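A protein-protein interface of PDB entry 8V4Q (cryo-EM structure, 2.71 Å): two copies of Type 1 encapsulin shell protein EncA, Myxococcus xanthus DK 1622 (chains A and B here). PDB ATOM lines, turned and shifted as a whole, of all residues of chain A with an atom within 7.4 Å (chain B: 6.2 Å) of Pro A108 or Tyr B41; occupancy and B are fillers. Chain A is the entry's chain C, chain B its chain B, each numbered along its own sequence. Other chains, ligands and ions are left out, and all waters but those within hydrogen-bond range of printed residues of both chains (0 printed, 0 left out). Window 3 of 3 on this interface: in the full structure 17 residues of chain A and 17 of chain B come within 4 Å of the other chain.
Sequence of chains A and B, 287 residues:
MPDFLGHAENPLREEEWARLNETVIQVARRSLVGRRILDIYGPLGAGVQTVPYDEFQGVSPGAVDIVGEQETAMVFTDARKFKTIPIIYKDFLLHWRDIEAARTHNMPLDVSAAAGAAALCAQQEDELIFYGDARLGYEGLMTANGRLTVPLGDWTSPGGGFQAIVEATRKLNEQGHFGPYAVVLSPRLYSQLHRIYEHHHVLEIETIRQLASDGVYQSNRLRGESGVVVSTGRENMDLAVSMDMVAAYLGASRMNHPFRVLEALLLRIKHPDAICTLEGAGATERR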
ATOM      1  N   ARG A  13      -2.809   4.334  13.498  1.00  0.00           N
ATOM      2  CA  ARG A  13      -3.977   4.627  14.310  1.00  0.00           C
ATOM      3  C   ARG A  13      -4.124   6.138  14.489  1.00  0.00           C
ATOM      4  O   ARG A  13      -3.389   6.936  13.903  1.00  0.00           O
ATOM      5  CB  ARG A  13      -3.879   3.913  15.656  1.00  0.00           C
ATOM      6  CG  ARG A  13      -3.967   2.397  15.561  1.00  0.00           C
ATOM      7  CD  ARG A  13      -3.503   1.728  16.847  1.00  0.00           C
ATOM      8  NE  ARG A  13      -2.088   1.966  17.109  1.00  0.00           N
ATOM      9  CZ  ARG A  13      -1.379   1.332  18.033  1.00  0.00           C
ATOM     10  NH1 ARG A  13      -1.923   0.409  18.809  1.00  0.00           N
ATOM     11  NH2 ARG A  13      -0.093   1.632  18.181  1.00  0.00           N
ATOM     12  N   GLU A  16      -1.132   7.598  16.830  1.00  0.00           N
ATOM     13  CA  GLU A  16       0.114   7.680  16.076  1.00  0.00           C
ATOM     14  C   GLU A  16       0.083   8.841  15.089  1.00  0.00           C
ATOM     15  O   GLU A  16       1.074   9.567  14.939  1.00  0.00           O
ATOM     16  CB  GLU A  16       0.373   6.358  15.353  1.00  0.00           C
ATOM     17  CG  GLU A  16       0.113   5.130  16.212  1.00  0.00           C
ATOM     18  CD  GLU A  16       0.449   3.833  15.503  1.00  0.00           C
ATOM     19  OE1 GLU A  16      -0.346   3.398  14.644  1.00  0.00           O
ATOM     20  OE2 GLU A  16       1.508   3.244  15.807  1.00  0.00           O
ATOM     21  N   ARG A  19       0.572  12.087  17.095  1.00  0.00           N
ATOM     22  CA  ARG A  19       1.970  12.244  17.545  1.00  0.00           C
ATOM     23  C   ARG A  19       2.921  12.503  16.384  1.00  0.00           C
ATOM     24  O   ARG A  19       3.955  13.083  16.640  1.00  0.00           O
ATOM     25  CB  ARG A  19       2.399  11.002  18.311  1.00  0.00           C
ATOM     26  CG  ARG A  19       2.957  11.316  19.690  1.00  0.00           C
ATOM     27  CD  ARG A  19       3.491  10.116  20.445  1.00  0.00           C
ATOM     28  NE  ARG A  19       4.881   9.799  20.153  1.00  0.00           N
ATOM     29  CZ  ARG A  19       5.283   8.649  19.637  1.00  0.00           C
ATOM     30  NH1 ARG A  19       4.397   7.709  19.356  1.00  0.00           N
ATOM     31  NH2 ARG A  19       6.562   8.440  19.404  1.00  0.00           N
ATOM     32  N   ASP A  98       8.178  -2.726  11.827  1.00  0.00           N
ATOM     33  CA  ASP A  98       8.219  -1.781  12.938  1.00  0.00           C
ATOM     34  C   ASP A  98       6.817  -1.426  13.416  1.00  0.00           C
ATOM     35  O   ASP A  98       6.566  -1.358  14.625  1.00  0.00           O
ATOM     36  CB  ASP A  98       8.980  -0.523  12.529  1.00  0.00           C
ATOM     37  CG  ASP A  98      10.476  -0.742  12.460  1.00  0.00           C
ATOM     38  OD1 ASP A  98      10.986  -1.607  13.199  1.00  0.00           O
ATOM     39  OD2 ASP A  98      11.144  -0.050  11.665  1.00  0.00           O
ATOM     40  N   ALA A 101       5.390  -4.452  15.254  1.00  0.00           N
ATOM     41  CA  ALA A 101       5.949  -4.547  16.599  1.00  0.00           C
ATOM     42  C   ALA A 101       5.374  -3.477  17.517  1.00  0.00           C
ATOM     43  O   ALA A 101       5.109  -3.740  18.695  1.00  0.00           O
ATOM     44  CB  ALA A 101       7.472  -4.442  16.543  1.00  0.00           C
ATOM     45  N   ALA A 102       5.185  -2.260  17.001  1.00  0.00           N
ATOM     46  CA  ALA A 102       4.633  -1.189  17.822  1.00  0.00           C
ATOM     47  C   ALA A 102       3.218  -1.512  18.279  1.00  0.00           C
ATOM     48  O   ALA A 102       2.868  -1.287  19.443  1.00  0.00           O
ATOM     49  CB  ALA A 102       4.662   0.131  17.053  1.00  0.00           C
ATOM     50  N   HIS A 105       3.612  -5.259  20.493  1.00  0.00           N
ATOM     51  CA  HIS A 105       4.384  -5.224  21.729  1.00  0.00           C
ATOM     52  C   HIS A 105       4.010  -4.061  22.637  1.00  0.00           C
ATOM     53  O   HIS A 105       4.531  -3.980  23.754  1.00  0.00           O
ATOM     54  CB  HIS A 105       5.884  -5.158  21.421  1.00  0.00           C
ATOM     55  CG  HIS A 105       6.397  -6.328  20.640  1.00  0.00           C
ATOM     56  ND1 HIS A 105       7.705  -6.426  20.220  1.00  0.00           N
ATOM     57  CD2 HIS A 105       5.777  -7.449  20.202  1.00  0.00           C
ATOM     58  CE1 HIS A 105       7.869  -7.556  19.557  1.00  0.00           C
ATOM     59  NE2 HIS A 105       6.715  -8.195  19.531  1.00  0.00           N
ATOM     60  N   ASN A 106       3.131  -3.165  22.183  1.00  0.00           N
ATOM     61  CA  ASN A 106       2.687  -2.003  22.954  1.00  0.00           C
ATOM     62  C   ASN A 106       3.869  -1.095  23.307  1.00  0.00           C
ATOM     63  O   ASN A 106       4.181  -0.850  24.473  1.00  0.00           O
ATOM     64  CB  ASN A 106       1.918  -2.438  24.208  1.00  0.00           C
ATOM     65  CG  ASN A 106       1.302  -1.270  24.954  1.00  0.00           C
ATOM     66  OD1 ASN A 106       1.593  -1.045  26.128  1.00  0.00           O
ATOM     67  ND2 ASN A 106       0.445  -0.519  24.272  1.00  0.00           N
ATOM     68  N   MET A 107       4.527  -0.599  22.265  1.00  0.00           N
ATOM     69  CA  MET A 107       5.653   0.308  22.410  1.00  0.00           C
ATOM     70  C   MET A 107       5.494   1.488  21.462  1.00  0.00           C
ATOM     71  O   MET A 107       4.896   1.352  20.390  1.00  0.00           O
ATOM     72  CB  MET A 107       6.984  -0.412  22.138  1.00  0.00           C
ATOM     73  CG  MET A 107       7.114  -1.007  20.748  1.00  0.00           C
ATOM     74  SD  MET A 107       8.375  -2.294  20.668  1.00  0.00           S
ATOM     75  CE  MET A 107       9.871  -1.318  20.777  1.00  0.00           C
ATOM     76  N   PRO A 108       6.008   2.659  21.836  1.00  0.00           N
ATOM     77  CA  PRO A 108       5.838   3.843  20.987  1.00  0.00           C
ATOM     78  C   PRO A 108       6.596   3.728  19.675  1.00  0.00           C
ATOM     79  O   PRO A 108       7.621   3.048  19.572  1.00  0.00           O
ATOM     80  CB  PRO A 108       6.395   4.982  21.851  1.00  0.00           C
ATOM     81  CG  PRO A 108       7.308   4.318  22.817  1.00  0.00           C
ATOM     82  CD  PRO A 108       6.708   2.974  23.093  1.00  0.00           C
ATOM     83  N   LEU A 109       6.072   4.408  18.661  1.00  0.00           N
ATOM     84  CA  LEU A 109       6.662   4.425  17.331  1.00  0.00           C
ATOM     85  C   LEU A 109       7.726   5.512  17.230  1.00  0.00           C
ATOM     86  O   LEU A 109       7.661   6.538  17.913  1.00  0.00           O
ATOM     87  CB  LEU A 109       5.580   4.645  16.272  1.00  0.00           C
ATOM     88  CG  LEU A 109       5.920   4.321  14.816  1.00  0.00           C
ATOM     89  CD1 LEU A 109       5.970   2.818  14.595  1.00  0.00           C
ATOM     90  CD2 LEU A 109       4.918   4.971  13.877  1.00  0.00           C
ATOM     91  N   ASP A 110       8.712   5.274  16.369  1.00  0.00           N
ATOM     92  CA  ASP A 110       9.815   6.204  16.162  1.00  0.00           C
ATOM     93  C   ASP A 110       9.472   7.179  15.041  1.00  0.00           C
ATOM     94  O   ASP A 110       9.059   6.762  13.954  1.00  0.00           O
ATOM     95  CB  ASP A 110      11.098   5.439  15.835  1.00  0.00           C
ATOM     96  CG  ASP A 110      12.347   6.244  16.120  1.00  0.00           C
ATOM     97  OD1 ASP A 110      12.277   7.187  16.933  1.00  0.00           O
ATOM     98  OD2 ASP A 110      13.401   5.931  15.531  1.00  0.00           O
ATOM     99  N   VAL A 111       9.648   8.475  15.307  1.00  0.00           N
ATOM    100  CA  VAL A 111       9.210   9.525  14.390  1.00  0.00           C
ATOM    101  C   VAL A 111      10.353  10.460  14.005  1.00  0.00           C
ATOM    102  O   VAL A 111      10.134  11.655  13.777  1.00  0.00           O
ATOM    103  CB  VAL A 111       8.040  10.321  15.000  1.00  0.00           C
ATOM    104  CG1 VAL A 111       6.792   9.460  15.071  1.00  0.00           C
ATOM    105  CG2 VAL A 111       8.409  10.828  16.386  1.00  0.00           C
ATOM    106  N   SER A 112      11.579   9.936  13.928  1.00  0.00           N
ATOM    107  CA  SER A 112      12.732  10.785  13.635  1.00  0.00           C
ATOM    108  C   SER A 112      12.813  11.188  12.165  1.00  0.00           C
ATOM    109  O   SER A 112      13.255  12.305  11.853  1.00  0.00           O
ATOM    110  CB  SER A 112      14.020  10.077  14.052  1.00  0.00           C
ATOM    111  OG  SER A 112      13.944   9.637  15.395  1.00  0.00           O
ATOM    112  N   ASP B  39      16.739  14.213  23.309  1.00  0.00           N
ATOM    113  CA  ASP B  39      15.383  13.701  23.197  1.00  0.00           C
ATOM    114  C   ASP B  39      15.317  12.260  23.696  1.00  0.00           C
ATOM    115  O   ASP B  39      16.315  11.535  23.718  1.00  0.00           O
ATOM    116  CB  ASP B  39      14.891  13.780  21.752  1.00  0.00           C
ATOM    117  CG  ASP B  39      14.397  15.162  21.378  1.00  0.00           C
ATOM    118  OD1 ASP B  39      13.573  15.724  22.128  1.00  0.00           O
ATOM    119  OD2 ASP B  39      14.833  15.689  20.333  1.00  0.00           O
ATOM    120  N   ILE B  40      14.117  11.847  24.095  1.00  0.00           N
ATOM    121  CA  ILE B  40      13.892  10.545  24.711  1.00  0.00           C
ATOM    122  C   ILE B  40      13.054   9.690  23.771  1.00  0.00           C
ATOM    123  O   ILE B  40      11.977  10.109  23.335  1.00  0.00           O
ATOM    124  CB  ILE B  40      13.204  10.676  26.082  1.00  0.00           C
ATOM    125  CG1 ILE B  40      14.076  11.482  27.047  1.00  0.00           C
ATOM    126  CG2 ILE B  40      12.887   9.304  26.656  1.00  0.00           C
ATOM    127  CD1 ILE B  40      15.405  10.836  27.355  1.00  0.00           C
ATOM    128  N   TYR B  41      13.551   8.495  23.466  1.00  0.00           N
ATOM    129  CA  TYR B  41      12.810   7.480  22.722  1.00  0.00           C
ATOM    130  C   TYR B  41      12.422   6.392  23.718  1.00  0.00           C
ATOM    131  O   TYR B  41      13.243   5.545  24.077  1.00  0.00           O
ATOM    132  CB  TYR B  41      13.645   6.926  21.571  1.00  0.00           C
ATOM    133  CG  TYR B  41      13.037   5.723  20.883  1.00  0.00           C
ATOM    134  CD1 TYR B  41      11.710   5.726  20.478  1.00  0.00           C
ATOM    135  CD2 TYR B  41      13.793   4.585  20.637  1.00  0.00           C
ATOM    136  CE1 TYR B  41      11.152   4.630  19.848  1.00  0.00           C
ATOM    137  CE2 TYR B  41      13.245   3.484  20.009  1.00  0.00           C
ATOM    138  CZ  TYR B  41      11.925   3.512  19.616  1.00  0.00           C
ATOM    139  OH  TYR B  41      11.375   2.418  18.990  1.00  0.00           O
ATOM    140  N   GLY B  42      11.172   6.426  24.171  1.00  0.00           N
ATOM    141  CA  GLY B  42      10.701   5.495  25.165  1.00  0.00           C
ATOM    142  C   GLY B  42       9.757   6.138  26.161  1.00  0.00           C
ATOM    143  O   GLY B  42       9.277   7.255  25.954  1.00  0.00           O
ATOM    144  N   PRO B  43       9.471   5.444  27.275  1.00  0.00           N
ATOM    145  CA  PRO B  43       9.972   4.115  27.675  1.00  0.00           C
ATOM    146  C   PRO B  43       9.429   2.987  26.805  1.00  0.00           C
ATOM    147  O   PRO B  43       8.270   2.997  26.403  1.00  0.00           O
ATOM    148  CB  PRO B  43       9.484   3.983  29.128  1.00  0.00           C
ATOM    149  CG  PRO B  43       9.242   5.388  29.590  1.00  0.00           C
ATOM    150  CD  PRO B  43       8.731   6.089  28.369  1.00  0.00           C
ATOM    151  N   LEU B  44      10.259   1.989  26.508  1.00  0.00           N
ATOM    152  CA  LEU B  44       9.873   0.902  25.621  1.00  0.00           C
ATOM    153  C   LEU B  44       9.400  -0.342  26.358  1.00  0.00           C
ATOM    154  O   LEU B  44       8.730  -1.183  25.751  1.00  0.00           O
ATOM    155  CB  LEU B  44      11.045   0.530  24.705  1.00  0.00           C
ATOM    156  CG  LEU B  44      11.719   1.706  23.993  1.00  0.00           C
ATOM    157  CD1 LEU B  44      13.063   1.297  23.410  1.00  0.00           C
ATOM    158  CD2 LEU B  44      10.813   2.274  22.913  1.00  0.00           C
ATOM    159  N   VAL B  51      18.024  -2.843  20.478  1.00  0.00           N
ATOM    160  CA  VAL B  51      17.462  -1.702  19.753  1.00  0.00           C
ATOM    161  C   VAL B  51      18.317  -1.416  18.531  1.00  0.00           C
ATOM    162  O   VAL B  51      19.545  -1.586  18.544  1.00  0.00           O
ATOM    163  CB  VAL B  51      17.376  -0.440  20.652  1.00  0.00           C
ATOM    164  CG1 VAL B  51      18.748   0.189  20.874  1.00  0.00           C
ATOM    165  CG2 VAL B  51      16.390   0.576  20.101  1.00  0.00           C
ATOM    166  N   ARG B 234      16.377  15.461  16.888  1.00  0.00           N
ATOM    167  CA  ARG B 234      16.021  14.058  17.072  1.00  0.00           C
ATOM    168  C   ARG B 234      16.653  13.169  16.009  1.00  0.00           C
ATOM    169  O   ARG B 234      16.942  11.997  16.273  1.00  0.00           O
ATOM    170  CB  ARG B 234      14.500  13.905  17.065  1.00  0.00           C
ATOM    171  CG  ARG B 234      14.002  12.522  17.430  1.00  0.00           C
ATOM    172  CD  ARG B 234      12.486  12.454  17.372  1.00  0.00           C
ATOM    173  NE  ARG B 234      11.858  13.292  18.385  1.00  0.00           N
ATOM    174  CZ  ARG B 234      11.640  12.918  19.639  1.00  0.00           C
ATOM    175  NH1 ARG B 234      11.998  11.722  20.076  1.00  0.00           N
ATOM    176  NH2 ARG B 234      11.048  13.765  20.475  1.00  0.00           N
ATOM    177  N   ASP B 238      19.680  10.855  20.109  1.00  0.00           N
ATOM    178  CA  ASP B 238      18.634  10.786  21.123  1.00  0.00           C
ATOM    179  C   ASP B 238      19.066   9.792  22.197  1.00  0.00           C
ATOM    180  O   ASP B 238      20.198   9.298  22.192  1.00  0.00           O
ATOM    181  CB  ASP B 238      17.279  10.425  20.499  1.00  0.00           C
ATOM    182  CG  ASP B 238      17.257   9.040  19.870  1.00  0.00           C
ATOM    183  OD1 ASP B 238      18.272   8.318  19.928  1.00  0.00           O
ATOM    184  OD2 ASP B 238      16.204   8.671  19.311  1.00  0.00           O
ATOM    185  N   LEU B 239      18.154   9.496  23.119  1.00  0.00           N
ATOM    186  CA  LEU B 239      18.404   8.559  24.206  1.00  0.00           C
ATOM    187  C   LEU B 239      17.282   7.534  24.223  1.00  0.00           C
ATOM    188  O   LEU B 239      16.116   7.891  24.415  1.00  0.00           O
ATOM    189  CB  LEU B 239      18.491   9.290  25.549  1.00  0.00           C
ATOM    190  CG  LEU B 239      19.151   8.555  26.715  1.00  0.00           C
ATOM    191  CD1 LEU B 239      20.640   8.391  26.465  1.00  0.00           C
ATOM    192  CD2 LEU B 239      18.900   9.294  28.017  1.00  0.00           C
ATOM    193  N   ALA B 240      17.632   6.264  24.023  1.00  0.00           N
ATOM    194  CA  ALA B 240      16.660   5.177  24.036  1.00  0.00           C
ATOM    195  C   ALA B 240      16.571   4.629  25.454  1.00  0.00           C
ATOM    196  O   ALA B 240      17.539   4.066  25.973  1.00  0.00           O
ATOM    197  CB  ALA B 240      17.053   4.086  23.044  1.00  0.00           C
ATOM    198  N   VAL B 241      15.408   4.786  26.079  1.00  0.00           N
ATOM    199  CA  VAL B 241      15.206   4.434  27.479  1.00  0.00           C
ATOM    200  C   VAL B 241      14.257   3.247  27.543  1.00  0.00           C
ATOM    201  O   VAL B 241      13.123   3.321  27.055  1.00  0.00           O
ATOM    202  CB  VAL B 241      14.658   5.619  28.288  1.00  0.00           C
ATOM    203  CG1 VAL B 241      14.532   5.246  29.755  1.00  0.00           C
ATOM    204  CG2 VAL B 241      15.547   6.840  28.113  1.00  0.00           C
ATOM    205  N   SER B 242      14.721   2.153  28.145  1.00  0.00           N
ATOM    206  CA  SER B 242      13.867   0.997  28.384  1.00  0.00           C
ATOM    207  C   SER B 242      13.174   1.064  29.737  1.00  0.00           C
ATOM    208  O   SER B 242      12.012   0.660  29.853  1.00  0.00           O
ATOM    209  CB  SER B 242      14.679  -0.296  28.283  1.00  0.00           C
ATOM    210  OG  SER B 242      15.083  -0.533  26.949  1.00  0.00           O
ATOM    211  N   ARG B 268      22.295   6.801  21.449  1.00  0.00           N
ATOM    212  CA  ARG B 268      22.425   6.520  20.023  1.00  0.00           C
ATOM    213  C   ARG B 268      22.962   7.754  19.312  1.00  0.00           C
ATOM    214  O   ARG B 268      22.326   8.813  19.335  1.00  0.00           O
ATOM    215  CB  ARG B 268      21.082   6.104  19.421  1.00  0.00           C
ATOM    216  CG  ARG B 268      20.297   5.120  20.266  1.00  0.00           C
ATOM    217  CD  ARG B 268      19.263   4.387  19.432  1.00  0.00           C
ATOM    218  NE  ARG B 268      18.078   5.200  19.192  1.00  0.00           N
ATOM    219  CZ  ARG B 268      17.069   4.839  18.411  1.00  0.00           C
ATOM    220  NH1 ARG B 268      17.070   3.680  17.773  1.00  0.00           N
ATOM    221  NH2 ARG B 268      16.035   5.661  18.265  1.00  0.00           N
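No position is printed for both chains.
NH2 of Arg B268 lies within salt-bridge range of OD2 of Asp B238 (3.2 Å).
The side-chain carboxylate of Asp B39 lies within salt-bridge range of the guanidinium group of Arg B234 (3.6 Å).
The side-chain hydroxyl (OG) of Ser A112 is in hydrogen-bond range of the side-chain carboxylate (OD1) of Asp A110 (3.3 Å).
N of Tyr B41 sits at hydrogen-bond distance from O of Leu B239 (2.8 Å).
The backbone carbonyl oxygen (O) of Tyr B41 lies within hydrogen-bond range of the backbone NH (N) of Val B241 (3.0 Å).
Among the printed residues, merely in contact across the chains: Ser A112 with Arg B234, Pro A108 with Pro B43, Pro A108 with Tyr B41 and Asp A110 with Tyr B41.
Hydrophobic or aromatic side chains of chain A that line the printed part of chain B: Pro A108.
Hydrophobic or aromatic side chains of chain B within 4 Å of the printed part of chain A: Tyr B41.
Among the printed residues, 5 pairs touch across the chains.
Among the printed residues, Asp or Glu carboxylates within 4 Å of a Lys or Arg side-chain nitrogen of the other chain: Asp A110 with Arg B268 (3.8 Å).
Of chain B, only Tyr B41 and Pro B43 come within 4 Å of Pro A108.
Tyr B41 touches just these residues of chain A: Pro A108 (3.9 Å) and Asp A110 (3.9 Å).
Of the printed residues of chain B, Asp A110 touches Tyr B41 and Arg B268.
Printed residues of chain B within 4 Å of Ser A112: Arg B234 (3.5 Å).
Of the printed residues of chain A, Pro B43 touches Pro A108 (3.7 Å).
Printed residues of chain A within 4 Å of Arg B268: Asp A110.
Of the printed residues of chain A, Arg B234 touches Ser A112 (3.5 Å).
Val A111 touches none of the printed residues of chain B.
The nearest residue of chain B that does not touch Pro A108 is Leu B44 (4.1 Å).
The nearest printed residue of chain A that does not touch Tyr B41 is Leu A109 (4.4 Å).
The side-chain carboxylate (OD2) of Asp A110 is in salt-bridge range of the guanidinium group (NH2) of Arg B268 (3.8 Å).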
